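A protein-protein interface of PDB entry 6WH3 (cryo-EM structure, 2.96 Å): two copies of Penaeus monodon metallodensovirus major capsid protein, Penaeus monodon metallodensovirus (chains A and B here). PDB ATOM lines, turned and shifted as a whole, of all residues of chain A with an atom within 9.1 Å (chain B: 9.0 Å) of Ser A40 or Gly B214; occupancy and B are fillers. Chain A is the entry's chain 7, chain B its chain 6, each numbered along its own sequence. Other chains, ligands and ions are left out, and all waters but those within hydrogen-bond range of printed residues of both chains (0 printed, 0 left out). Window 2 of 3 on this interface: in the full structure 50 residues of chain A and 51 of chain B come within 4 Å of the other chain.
Among the printed residues, pairs that only touch across the chains: Trp A47 with Asn B130, Ser A40 with Asp B215, Gly A37 with Asp B216, Ser A40 with Gly B214, Ala A41 with Gly B214 and Trp A47 with Thr B292.
Printed residues of chain B within 4 Å of Ser A40: Asn B130 (3.4 Å), Gly B214 (3.6 Å) and Asp B215 (3.3 Å).
Of chain A, only Ser A40 (3.6 Å) and Ala A41 (3.7 Å) come within 4 Å of Gly B214.
Of chain B, only Asp B216 and Ala B217 come within 4 Å of Asp A38.
No residue of chain B comes within 4 Å of Gly A39.
Of the printed residues of chain B, Ala A41 touches Gly B214 (3.7 Å).
Of the printed residues of chain A, Asn B130 touches Ser A40 (3.4 Å) and Trp A47 (2.8 Å).
Of the printed residues of chain B, Gly A37 touches Asp B216 (3.5 Å).
The nearest residue of chain B that does not touch Ser A40 is Ala B217 (4.1 Å).
The nearest printed residue of chain A that does not touch Ala B217 is Ser A40 (4.1 Å).
OD1 of Asp A38 sits at hydrogen-bond distance from OG of Ser A40, 2.7 Å away.
OG of Ser B129 is in hydrogen-bond range of OD1 of Asn B130, at 3.1 Å.
The backbone NH (N) of Thr B292 sits at hydrogen-bond distance from the backbone carbonyl oxygen (O) of Ser B129 (2.9 Å).
O of Asp B216 lies within hydrogen-bond range of NE1 of Trp B211 (2.9 Å).
N of Lys B212 lies within hydrogen-bond range of OD2 of Asp B215.
No position is printed for both chains.
Of the 10 pairs that touch across the chains among the printed residues, none has its exchanged pair printed and touching as well.
Printed residues of chain B that touch a printed residue of chain A: Ser B129, Asn B130, Gly B214, Asp B215, Asp B216, Ala B217 and Thr B292.
Of the 13 printed residues of chain A, 5 touch a printed residue of chain B.
Hydrophobic or aromatic side chains of chain A within 4 Å of the printed part of chain B: Trp A47.
Among the printed residues, 10 pairs touch across the chains.
Among the printed residues, no Asp or Glu carboxylate lies within 4 Å of a Lys or Arg side-chain nitrogen of the other chain.
The side-chain hydroxyl (OG) of Ser A40 lies close to the side-chain amide nitrogen (ND2) of Asn B130, at 3.5 Å.
The backbone NH (N) of Ala B217 sits at hydrogen-bond distance from the side-chain carboxylate (OD2) of Asp A38 (2.7 Å).
The side-chain hydroxyl (OG) of Ser B129 sits close to the indole nitrogen (NE1) of Trp A47 (3.4 Å).
N of Asp A38 lies within hydrogen-bond range of OD1 of Asp B216 (3.2 Å).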
ATOM      1  N   GLU A  36      25.397  15.211   4.359  1.00  0.00           N
ATOM      2  CA  GLU A  36      25.236  16.057   3.185  1.00  0.00           C
ATOM      3  C   GLU A  36      25.295  15.195   1.929  1.00  0.00           C
ATOM      4  O   GLU A  36      25.886  14.116   1.943  1.00  0.00           O
ATOM      5  CB  GLU A  36      26.314  17.146   3.159  1.00  0.00           C
ATOM      6  CG  GLU A  36      26.185  18.161   2.030  1.00  0.00           C
ATOM      7  CD  GLU A  36      24.947  19.032   2.152  1.00  0.00           C
ATOM      8  OE1 GLU A  36      24.324  19.048   3.234  1.00  0.00           O
ATOM      9  OE2 GLU A  36      24.594  19.701   1.160  1.00  0.00           O
ATOM     10  N   GLY A  37      24.676  15.661   0.850  1.00  0.00           N
ATOM     11  CA  GLY A  37      24.647  14.907  -0.384  1.00  0.00           C
ATOM     12  C   GLY A  37      23.499  13.925  -0.420  1.00  0.00           C
ATOM     13  O   GLY A  37      22.662  13.849   0.480  1.00  0.00           O
ATOM     14  N   ASP A  38      23.465  13.145  -1.492  1.00  0.00           N
ATOM     15  CA  ASP A  38      22.426  12.144  -1.665  1.00  0.00           C
ATOM     16  C   ASP A  38      22.752  10.831  -0.973  1.00  0.00           C
ATOM     17  O   ASP A  38      21.966   9.886  -1.070  1.00  0.00           O
ATOM     18  CB  ASP A  38      22.155  11.905  -3.155  1.00  0.00           C
ATOM     19  CG  ASP A  38      23.348  11.343  -3.895  1.00  0.00           C
ATOM     20  OD1 ASP A  38      24.350  10.968  -3.263  1.00  0.00           O
ATOM     21  OD2 ASP A  38      23.275  11.274  -5.134  1.00  0.00           O
ATOM     22  N   GLY A  39      23.887  10.751  -0.288  1.00  0.00           N
ATOM     23  CA  GLY A  39      24.293   9.560   0.423  1.00  0.00           C
ATOM     24  C   GLY A  39      25.421   8.805  -0.228  1.00  0.00           C
ATOM     25  O   GLY A  39      26.019   7.944   0.423  1.00  0.00           O
ATOM     26  N   SER A  40      25.711   9.118  -1.485  1.00  0.00           N
ATOM     27  CA  SER A  40      26.739   8.438  -2.263  1.00  0.00           C
ATOM     28  C   SER A  40      28.141   8.541  -1.716  1.00  0.00           C
ATOM     29  O   SER A  40      29.030   7.855  -2.187  1.00  0.00           O
ATOM     30  CB  SER A  40      26.739   8.946  -3.700  1.00  0.00           C
ATOM     31  OG  SER A  40      25.478   8.775  -4.303  1.00  0.00           O
ATOM     32  N   ALA A  41      28.338   9.374  -0.704  1.00  0.00           N
ATOM     33  CA  ALA A  41      29.647   9.580  -0.093  1.00  0.00           C
ATOM     34  C   ALA A  41      30.086   8.411   0.770  1.00  0.00           C
ATOM     35  O   ALA A  41      29.306   7.552   1.101  1.00  0.00           O
ATOM     36  CB  ALA A  41      29.655  10.862   0.710  1.00  0.00           C
ATOM     37  N   PRO A  42      31.365   8.345   1.105  1.00  0.00           N
ATOM     38  CA  PRO A  42      31.784   7.220   1.934  1.00  0.00           C
ATOM     39  C   PRO A  42      31.117   7.135   3.306  1.00  0.00           C
ATOM     40  O   PRO A  42      30.847   6.027   3.714  1.00  0.00           O
ATOM     41  CB  PRO A  42      33.279   7.430   2.046  1.00  0.00           C
ATOM     42  CG  PRO A  42      33.627   8.014   0.723  1.00  0.00           C
ATOM     43  CD  PRO A  42      32.508   8.968   0.426  1.00  0.00           C
ATOM     44  N   GLY A  43      30.850   8.229   4.002  1.00  0.00           N
ATOM     45  CA  GLY A  43      30.247   8.134   5.326  1.00  0.00           C
ATOM     46  C   GLY A  43      28.871   8.758   5.492  1.00  0.00           C
ATOM     47  O   GLY A  43      28.492   9.618   4.713  1.00  0.00           O
ATOM     48  N   GLY A  44      28.117   8.340   6.504  1.00  0.00           N
ATOM     49  CA  GLY A  44      26.783   8.876   6.722  1.00  0.00           C
ATOM     50  C   GLY A  44      25.650   7.959   6.307  1.00  0.00           C
ATOM     51  O   GLY A  44      25.639   6.802   6.677  1.00  0.00           O
ATOM     52  N   SER A  45      24.672   8.484   5.582  1.00  0.00           N
ATOM     53  CA  SER A  45      23.525   7.708   5.124  1.00  0.00           C
ATOM     54  C   SER A  45      23.772   6.895   3.852  1.00  0.00           C
ATOM     55  O   SER A  45      24.553   7.261   3.029  1.00  0.00           O
ATOM     56  CB  SER A  45      22.344   8.639   4.910  1.00  0.00           C
ATOM     57  OG  SER A  45      21.141   7.907   4.806  1.00  0.00           O
ATOM     58  N   VAL A  46      23.043   5.808   3.682  1.00  0.00           N
ATOM     59  CA  VAL A  46      23.157   4.886   2.562  1.00  0.00           C
ATOM     60  C   VAL A  46      22.452   5.386   1.325  1.00  0.00           C
ATOM     61  O   VAL A  46      21.310   5.800   1.390  1.00  0.00           O
ATOM     62  CB  VAL A  46      22.689   3.482   2.950  1.00  0.00           C
ATOM     63  CG1 VAL A  46      22.143   2.739   1.753  1.00  0.00           C
ATOM     64  CG2 VAL A  46      23.827   2.718   3.588  1.00  0.00           C
ATOM     65  N   TRP A  47      23.157   5.407   0.203  1.00  0.00           N
ATOM     66  CA  TRP A  47      22.524   5.803  -1.034  1.00  0.00           C
ATOM     67  C   TRP A  47      21.661   4.619  -1.364  1.00  0.00           C
ATOM     68  O   TRP A  47      22.140   3.499  -1.376  1.00  0.00           O
ATOM     69  CB  TRP A  47      23.527   6.002  -2.158  1.00  0.00           C
ATOM     70  CG  TRP A  47      22.847   6.389  -3.417  1.00  0.00           C
ATOM     71  CD1 TRP A  47      22.536   7.643  -3.819  1.00  0.00           C
ATOM     72  CD2 TRP A  47      22.343   5.509  -4.424  1.00  0.00           C
ATOM     73  NE1 TRP A  47      21.887   7.609  -5.022  1.00  0.00           N
ATOM     74  CE2 TRP A  47      21.753   6.305  -5.411  1.00  0.00           C
ATOM     75  CE3 TRP A  47      22.336   4.126  -4.585  1.00  0.00           C
ATOM     76  CZ2 TRP A  47      21.168   5.766  -6.540  1.00  0.00           C
ATOM     77  CZ3 TRP A  47      21.757   3.600  -5.702  1.00  0.00           C
ATOM     78  CH2 TRP A  47      21.183   4.411  -6.665  1.00  0.00           C
ATOM     79  N   GLN A  48      20.389   4.845  -1.631  1.00  0.00           N
ATOM     80  CA  GLN A  48      19.514   3.730  -1.928  1.00  0.00           C
ATOM     81  C   GLN A  48      18.737   3.996  -3.204  1.00  0.00           C
ATOM     82  O   GLN A  48      18.460   5.141  -3.563  1.00  0.00           O
ATOM     83  CB  GLN A  48      18.573   3.436  -0.770  1.00  0.00           C
ATOM     84  CG  GLN A  48      17.619   4.530  -0.430  1.00  0.00           C
ATOM     85  CD  GLN A  48      16.751   4.151   0.731  1.00  0.00           C
ATOM     86  OE1 GLN A  48      17.089   3.257   1.497  1.00  0.00           O
ATOM     87  NE2 GLN A  48      15.621   4.825   0.872  1.00  0.00           N
ATOM     88  N   THR B 127      19.821   7.901 -14.598  1.00  0.00           N
ATOM     89  CA  THR B 127      20.661   8.307 -13.483  1.00  0.00           C
ATOM     90  C   THR B 127      21.923   7.463 -13.445  1.00  0.00           C
ATOM     91  O   THR B 127      21.855   6.237 -13.548  1.00  0.00           O
ATOM     92  CB  THR B 127      19.916   8.170 -12.156  1.00  0.00           C
ATOM     93  OG1 THR B 127      18.771   9.029 -12.157  1.00  0.00           O
ATOM     94  CG2 THR B 127      20.807   8.537 -11.007  1.00  0.00           C
ATOM     95  N   LEU B 128      23.065   8.122 -13.308  1.00  0.00           N
ATOM     96  CA  LEU B 128      24.337   7.482 -13.009  1.00  0.00           C
ATOM     97  C   LEU B 128      24.653   7.688 -11.541  1.00  0.00           C
ATOM     98  O   LEU B 128      24.577   8.813 -11.044  1.00  0.00           O
ATOM     99  CB  LEU B 128      25.449   8.069 -13.870  1.00  0.00           C
ATOM    100  CG  LEU B 128      25.747   7.420 -15.209  1.00  0.00           C
ATOM    101  CD1 LEU B 128      24.558   7.447 -16.087  1.00  0.00           C
ATOM    102  CD2 LEU B 128      26.862   8.191 -15.857  1.00  0.00           C
ATOM    103  N   SER B 129      25.016   6.615 -10.849  1.00  0.00           N
ATOM    104  CA  SER B 129      25.127   6.698  -9.405  1.00  0.00           C
ATOM    105  C   SER B 129      26.244   5.808  -8.893  1.00  0.00           C
ATOM    106  O   SER B 129      26.577   4.793  -9.505  1.00  0.00           O
ATOM    107  CB  SER B 129      23.816   6.306  -8.741  1.00  0.00           C
ATOM    108  OG  SER B 129      23.969   6.327  -7.342  1.00  0.00           O
ATOM    109  N   ASN B 130      26.810   6.204  -7.754  1.00  0.00           N
ATOM    110  CA  ASN B 130      27.787   5.416  -7.002  1.00  0.00           C
ATOM    111  C   ASN B 130      28.907   4.904  -7.898  1.00  0.00           C
ATOM    112  O   ASN B 130      29.045   3.719  -8.179  1.00  0.00           O
ATOM    113  CB  ASN B 130      27.092   4.279  -6.266  1.00  0.00           C
ATOM    114  CG  ASN B 130      26.231   4.784  -5.168  1.00  0.00           C
ATOM    115  OD1 ASN B 130      25.059   4.478  -5.103  1.00  0.00           O
ATOM    116  ND2 ASN B 130      26.818   5.546  -4.264  1.00  0.00           N
ATOM    117  N   LEU B 131      29.714   5.863  -8.322  1.00  0.00           N
ATOM    118  CA  LEU B 131      30.827   5.578  -9.200  1.00  0.00           C
ATOM    119  C   LEU B 131      31.936   4.873  -8.442  1.00  0.00           C
ATOM    120  O   LEU B 131      32.277   5.245  -7.319  1.00  0.00           O
ATOM    121  CB  LEU B 131      31.341   6.872  -9.801  1.00  0.00           C
ATOM    122  CG  LEU B 131      32.521   6.766 -10.740  1.00  0.00           C
ATOM    123  CD1 LEU B 131      32.180   5.949 -11.953  1.00  0.00           C
ATOM    124  CD2 LEU B 131      32.891   8.142 -11.143  1.00  0.00           C
ATOM    125  N   ILE B 132      32.491   3.840  -9.060  1.00  0.00           N
ATOM    126  CA  ILE B 132      33.650   3.133  -8.539  1.00  0.00           C
ATOM    127  C   ILE B 132      34.684   3.097  -9.647  1.00  0.00           C
ATOM    128  O   ILE B 132      34.451   2.486 -10.694  1.00  0.00           O
ATOM    129  CB  ILE B 132      33.318   1.706  -8.086  1.00  0.00           C
ATOM    130  CG1 ILE B 132      32.363   1.714  -6.905  1.00  0.00           C
ATOM    131  CG2 ILE B 132      34.571   0.988  -7.697  1.00  0.00           C
ATOM    132  CD1 ILE B 132      31.833   0.350  -6.570  1.00  0.00           C
ATOM    133  N   LEU B 133      35.815   3.749  -9.421  1.00  0.00           N
ATOM    134  CA  LEU B 133      36.955   3.687 -10.318  1.00  0.00           C
ATOM    135  C   LEU B 133      37.944   2.647  -9.827  1.00  0.00           C
ATOM    136  O   LEU B 133      38.223   2.555  -8.632  1.00  0.00           O
ATOM    137  CB  LEU B 133      37.661   5.035 -10.426  1.00  0.00           C
ATOM    138  CG  LEU B 133      37.178   6.020 -11.474  1.00  0.00           C
ATOM    139  CD1 LEU B 133      35.831   6.421 -11.136  1.00  0.00           C
ATOM    140  CD2 LEU B 133      38.052   7.223 -11.456  1.00  0.00           C
ATOM    141  N   THR B 153      40.896   9.270  -4.417  1.00  0.00           N
ATOM    142  CA  THR B 153      39.655   9.575  -5.109  1.00  0.00           C
ATOM    143  C   THR B 153      39.790  10.719  -6.099  1.00  0.00           C
ATOM    144  O   THR B 153      38.782  11.150  -6.666  1.00  0.00           O
ATOM    145  CB  THR B 153      38.561   9.878  -4.091  1.00  0.00           C
ATOM    146  OG1 THR B 153      38.996  10.927  -3.225  1.00  0.00           O
ATOM    147  CG2 THR B 153      38.256   8.647  -3.270  1.00  0.00           C
ATOM    148  N   PRO B 155      40.973  10.700  -9.212  1.00  0.00           N
ATOM    149  CA  PRO B 155      40.548  10.420 -10.584  1.00  0.00           C
ATOM    150  C   PRO B 155      39.044  10.554 -10.737  1.00  0.00           C
ATOM    151  O   PRO B 155      38.285  10.520  -9.770  1.00  0.00           O
ATOM    152  CB  PRO B 155      40.995   8.975 -10.803  1.00  0.00           C
ATOM    153  CG  PRO B 155      42.079   8.787  -9.887  1.00  0.00           C
ATOM    154  CD  PRO B 155      41.695   9.542  -8.665  1.00  0.00           C
ATOM    155  N   TRP B 211      33.185  13.579 -12.689  1.00  0.00           N
ATOM    156  CA  TRP B 211      32.398  12.920 -11.665  1.00  0.00           C
ATOM    157  C   TRP B 211      33.278  11.902 -10.971  1.00  0.00           C
ATOM    158  O   TRP B 211      33.791  10.980 -11.604  1.00  0.00           O
ATOM    159  CB  TRP B 211      31.136  12.325 -12.289  1.00  0.00           C
ATOM    160  CG  TRP B 211      30.239  11.549 -11.396  1.00  0.00           C
ATOM    161  CD1 TRP B 211      29.512  12.032 -10.361  1.00  0.00           C
ATOM    162  CD2 TRP B 211      29.740  10.232 -11.641  1.00  0.00           C
ATOM    163  NE1 TRP B 211      28.719  11.051  -9.840  1.00  0.00           N
ATOM    164  CE2 TRP B 211      28.826   9.939 -10.628  1.00  0.00           C
ATOM    165  CE3 TRP B 211      30.024   9.254 -12.589  1.00  0.00           C
ATOM    166  CZ2 TRP B 211      28.194   8.712 -10.531  1.00  0.00           C
ATOM    167  CZ3 TRP B 211      29.403   8.042 -12.487  1.00  0.00           C
ATOM    168  CH2 TRP B 211      28.498   7.778 -11.469  1.00  0.00           C
ATOM    169  N   LYS B 212      33.487  12.111  -9.681  1.00  0.00           N
ATOM    170  CA  LYS B 212      34.454  11.366  -8.906  1.00  0.00           C
ATOM    171  C   LYS B 212      33.755  10.344  -8.027  1.00  0.00           C
ATOM    172  O   LYS B 212      32.533  10.202  -8.027  1.00  0.00           O
ATOM    173  CB  LYS B 212      35.294  12.316  -8.057  1.00  0.00           C
ATOM    174  CG  LYS B 212      36.159  13.244  -8.859  1.00  0.00           C
ATOM    175  CD  LYS B 212      36.918  14.189  -7.975  1.00  0.00           C
ATOM    176  CE  LYS B 212      37.804  15.086  -8.802  1.00  0.00           C
ATOM    177  NZ  LYS B 212      38.540  16.066  -7.966  1.00  0.00           N
ATOM    178  N   GLN B 213      34.555   9.627  -7.259  1.00  0.00           N
ATOM    179  CA  GLN B 213      34.046   8.666  -6.301  1.00  0.00           C
ATOM    180  C   GLN B 213      33.515   9.414  -5.089  1.00  0.00           C
ATOM    181  O   GLN B 213      34.253  10.166  -4.445  1.00  0.00           O
ATOM    182  CB  GLN B 213      35.168   7.718  -5.915  1.00  0.00           C
ATOM    183  CG  GLN B 213      35.629   6.839  -7.036  1.00  0.00           C
ATOM    184  CD  GLN B 213      36.883   6.103  -6.674  1.00  0.00           C
ATOM    185  OE1 GLN B 213      37.674   6.580  -5.874  1.00  0.00           O
ATOM    186  NE2 GLN B 213      37.063   4.927  -7.232  1.00  0.00           N
ATOM    187  N   GLY B 214      32.247   9.208  -4.771  1.00  0.00           N
ATOM    188  CA  GLY B 214      31.603   9.899  -3.686  1.00  0.00           C
ATOM    189  C   GLY B 214      30.714  11.042  -4.114  1.00  0.00           C
ATOM    190  O   GLY B 214      29.908  11.511  -3.309  1.00  0.00           O
ATOM    191  N   ASP B 215      30.840  11.503  -5.353  1.00  0.00           N
ATOM    192  CA  ASP B 215      29.966  12.553  -5.842  1.00  0.00           C
ATOM    193  C   ASP B 215      28.526  12.068  -5.899  1.00  0.00           C
ATOM    194  O   ASP B 215      28.245  10.873  -5.968  1.00  0.00           O
ATOM    195  CB  ASP B 215      30.407  13.031  -7.221  1.00  0.00           C
ATOM    196  CG  ASP B 215      31.594  13.950  -7.165  1.00  0.00           C
ATOM    197  OD1 ASP B 215      31.861  14.517  -6.093  1.00  0.00           O
ATOM    198  OD2 ASP B 215      32.270  14.108  -8.195  1.00  0.00           O
ATOM    199  N   ASP B 216      27.608  13.022  -5.861  1.00  0.00           N
ATOM    200  CA  ASP B 216      26.200  12.698  -5.927  1.00  0.00           C
ATOM    201  C   ASP B 216      25.865  12.113  -7.288  1.00  0.00           C
ATOM    202  O   ASP B 216      26.593  12.288  -8.265  1.00  0.00           O
ATOM    203  CB  ASP B 216      25.352  13.939  -5.671  1.00  0.00           C
ATOM    204  CG  ASP B 216      25.437  14.417  -4.248  1.00  0.00           C
ATOM    205  OD1 ASP B 216      25.936  13.658  -3.394  1.00  0.00           O
ATOM    206  OD2 ASP B 216      24.988  15.549  -3.976  1.00  0.00           O
ATOM    207  N   ALA B 217      24.751  11.397  -7.340  1.00  0.00           N
ATOM    208  CA  ALA B 217      24.326  10.776  -8.582  1.00  0.00           C
ATOM    209  C   ALA B 217      24.071  11.832  -9.646  1.00  0.00           C
ATOM    210  O   ALA B 217      23.703  12.968  -9.352  1.00  0.00           O
ATOM    211  CB  ALA B 217      23.069   9.947  -8.353  1.00  0.00           C
ATOM    212  N   LEU B 218      24.284  11.447 -10.896  1.00  0.00           N
ATOM    213  CA  LEU B 218      24.081  12.326 -12.036  1.00  0.00           C
ATOM    214  C   LEU B 218      22.733  12.012 -12.662  1.00  0.00           C
ATOM    215  O   LEU B 218      22.529  10.911 -13.175  1.00  0.00           O
ATOM    216  CB  LEU B 218      25.195  12.151 -13.061  1.00  0.00           C
ATOM    217  CG  LEU B 218      26.603  12.529 -12.633  1.00  0.00           C
ATOM    218  CD1 LEU B 218      27.561  12.196 -13.743  1.00  0.00           C
ATOM    219  CD2 LEU B 218      26.670  13.989 -12.292  1.00  0.00           C
ATOM    220  N   HIS B 219      21.823  12.976 -12.627  1.00  0.00           N
ATOM    221  CA  HIS B 219      20.459  12.786 -13.091  1.00  0.00           C
ATOM    222  C   HIS B 219      20.271  13.518 -14.405  1.00  0.00           C
ATOM    223  O   HIS B 219      20.575  14.710 -14.499  1.00  0.00           O
ATOM    224  CB  HIS B 219      19.466  13.311 -12.060  1.00  0.00           C
ATOM    225  CG  HIS B 219      19.634  12.710 -10.704  1.00  0.00           C
ATOM    226  ND1 HIS B 219      19.322  11.399 -10.425  1.00  0.00           N
ATOM    227  CD2 HIS B 219      20.101  13.241  -9.551  1.00  0.00           C
ATOM    228  CE1 HIS B 219      19.582  11.150  -9.156  1.00  0.00           C
ATOM    229  NE2 HIS B 219      20.055  12.250  -8.603  1.00  0.00           N
ATOM    230  N   GLN B 290      32.817   1.706 -12.534  1.00  0.00           N
ATOM    231  CA  GLN B 290      31.515   1.116 -12.291  1.00  0.00           C
ATOM    232  C   GLN B 290      30.558   2.200 -11.838  1.00  0.00           C
ATOM    233  O   GLN B 290      30.943   3.115 -11.113  1.00  0.00           O
ATOM    234  CB  GLN B 290      31.507   0.077 -11.202  1.00  0.00           C
ATOM    235  CG  GLN B 290      30.169  -0.599 -11.182  1.00  0.00           C
ATOM    236  CD  GLN B 290      29.969  -1.472 -10.016  1.00  0.00           C
ATOM    237  OE1 GLN B 290      30.817  -1.558  -9.152  1.00  0.00           O
ATOM    238  NE2 GLN B 290      28.841  -2.148  -9.978  1.00  0.00           N
ATOM    239  N   THR B 292      25.902   2.556 -11.208  1.00  0.00           N
ATOM    240  CA  THR B 292      24.577   2.008 -11.421  1.00  0.00           C
ATOM    241  C   THR B 292      23.829   2.887 -12.406  1.00  0.00           C
ATOM    242  O   THR B 292      23.886   4.114 -12.325  1.00  0.00           O
ATOM    243  CB  THR B 292      23.795   1.919 -10.116  1.00  0.00           C
ATOM    244  OG1 THR B 292      23.613   3.230  -9.587  1.00  0.00           O
ATOM    245  CG2 THR B 292      24.571   1.130  -9.124  1.00  0.00           C
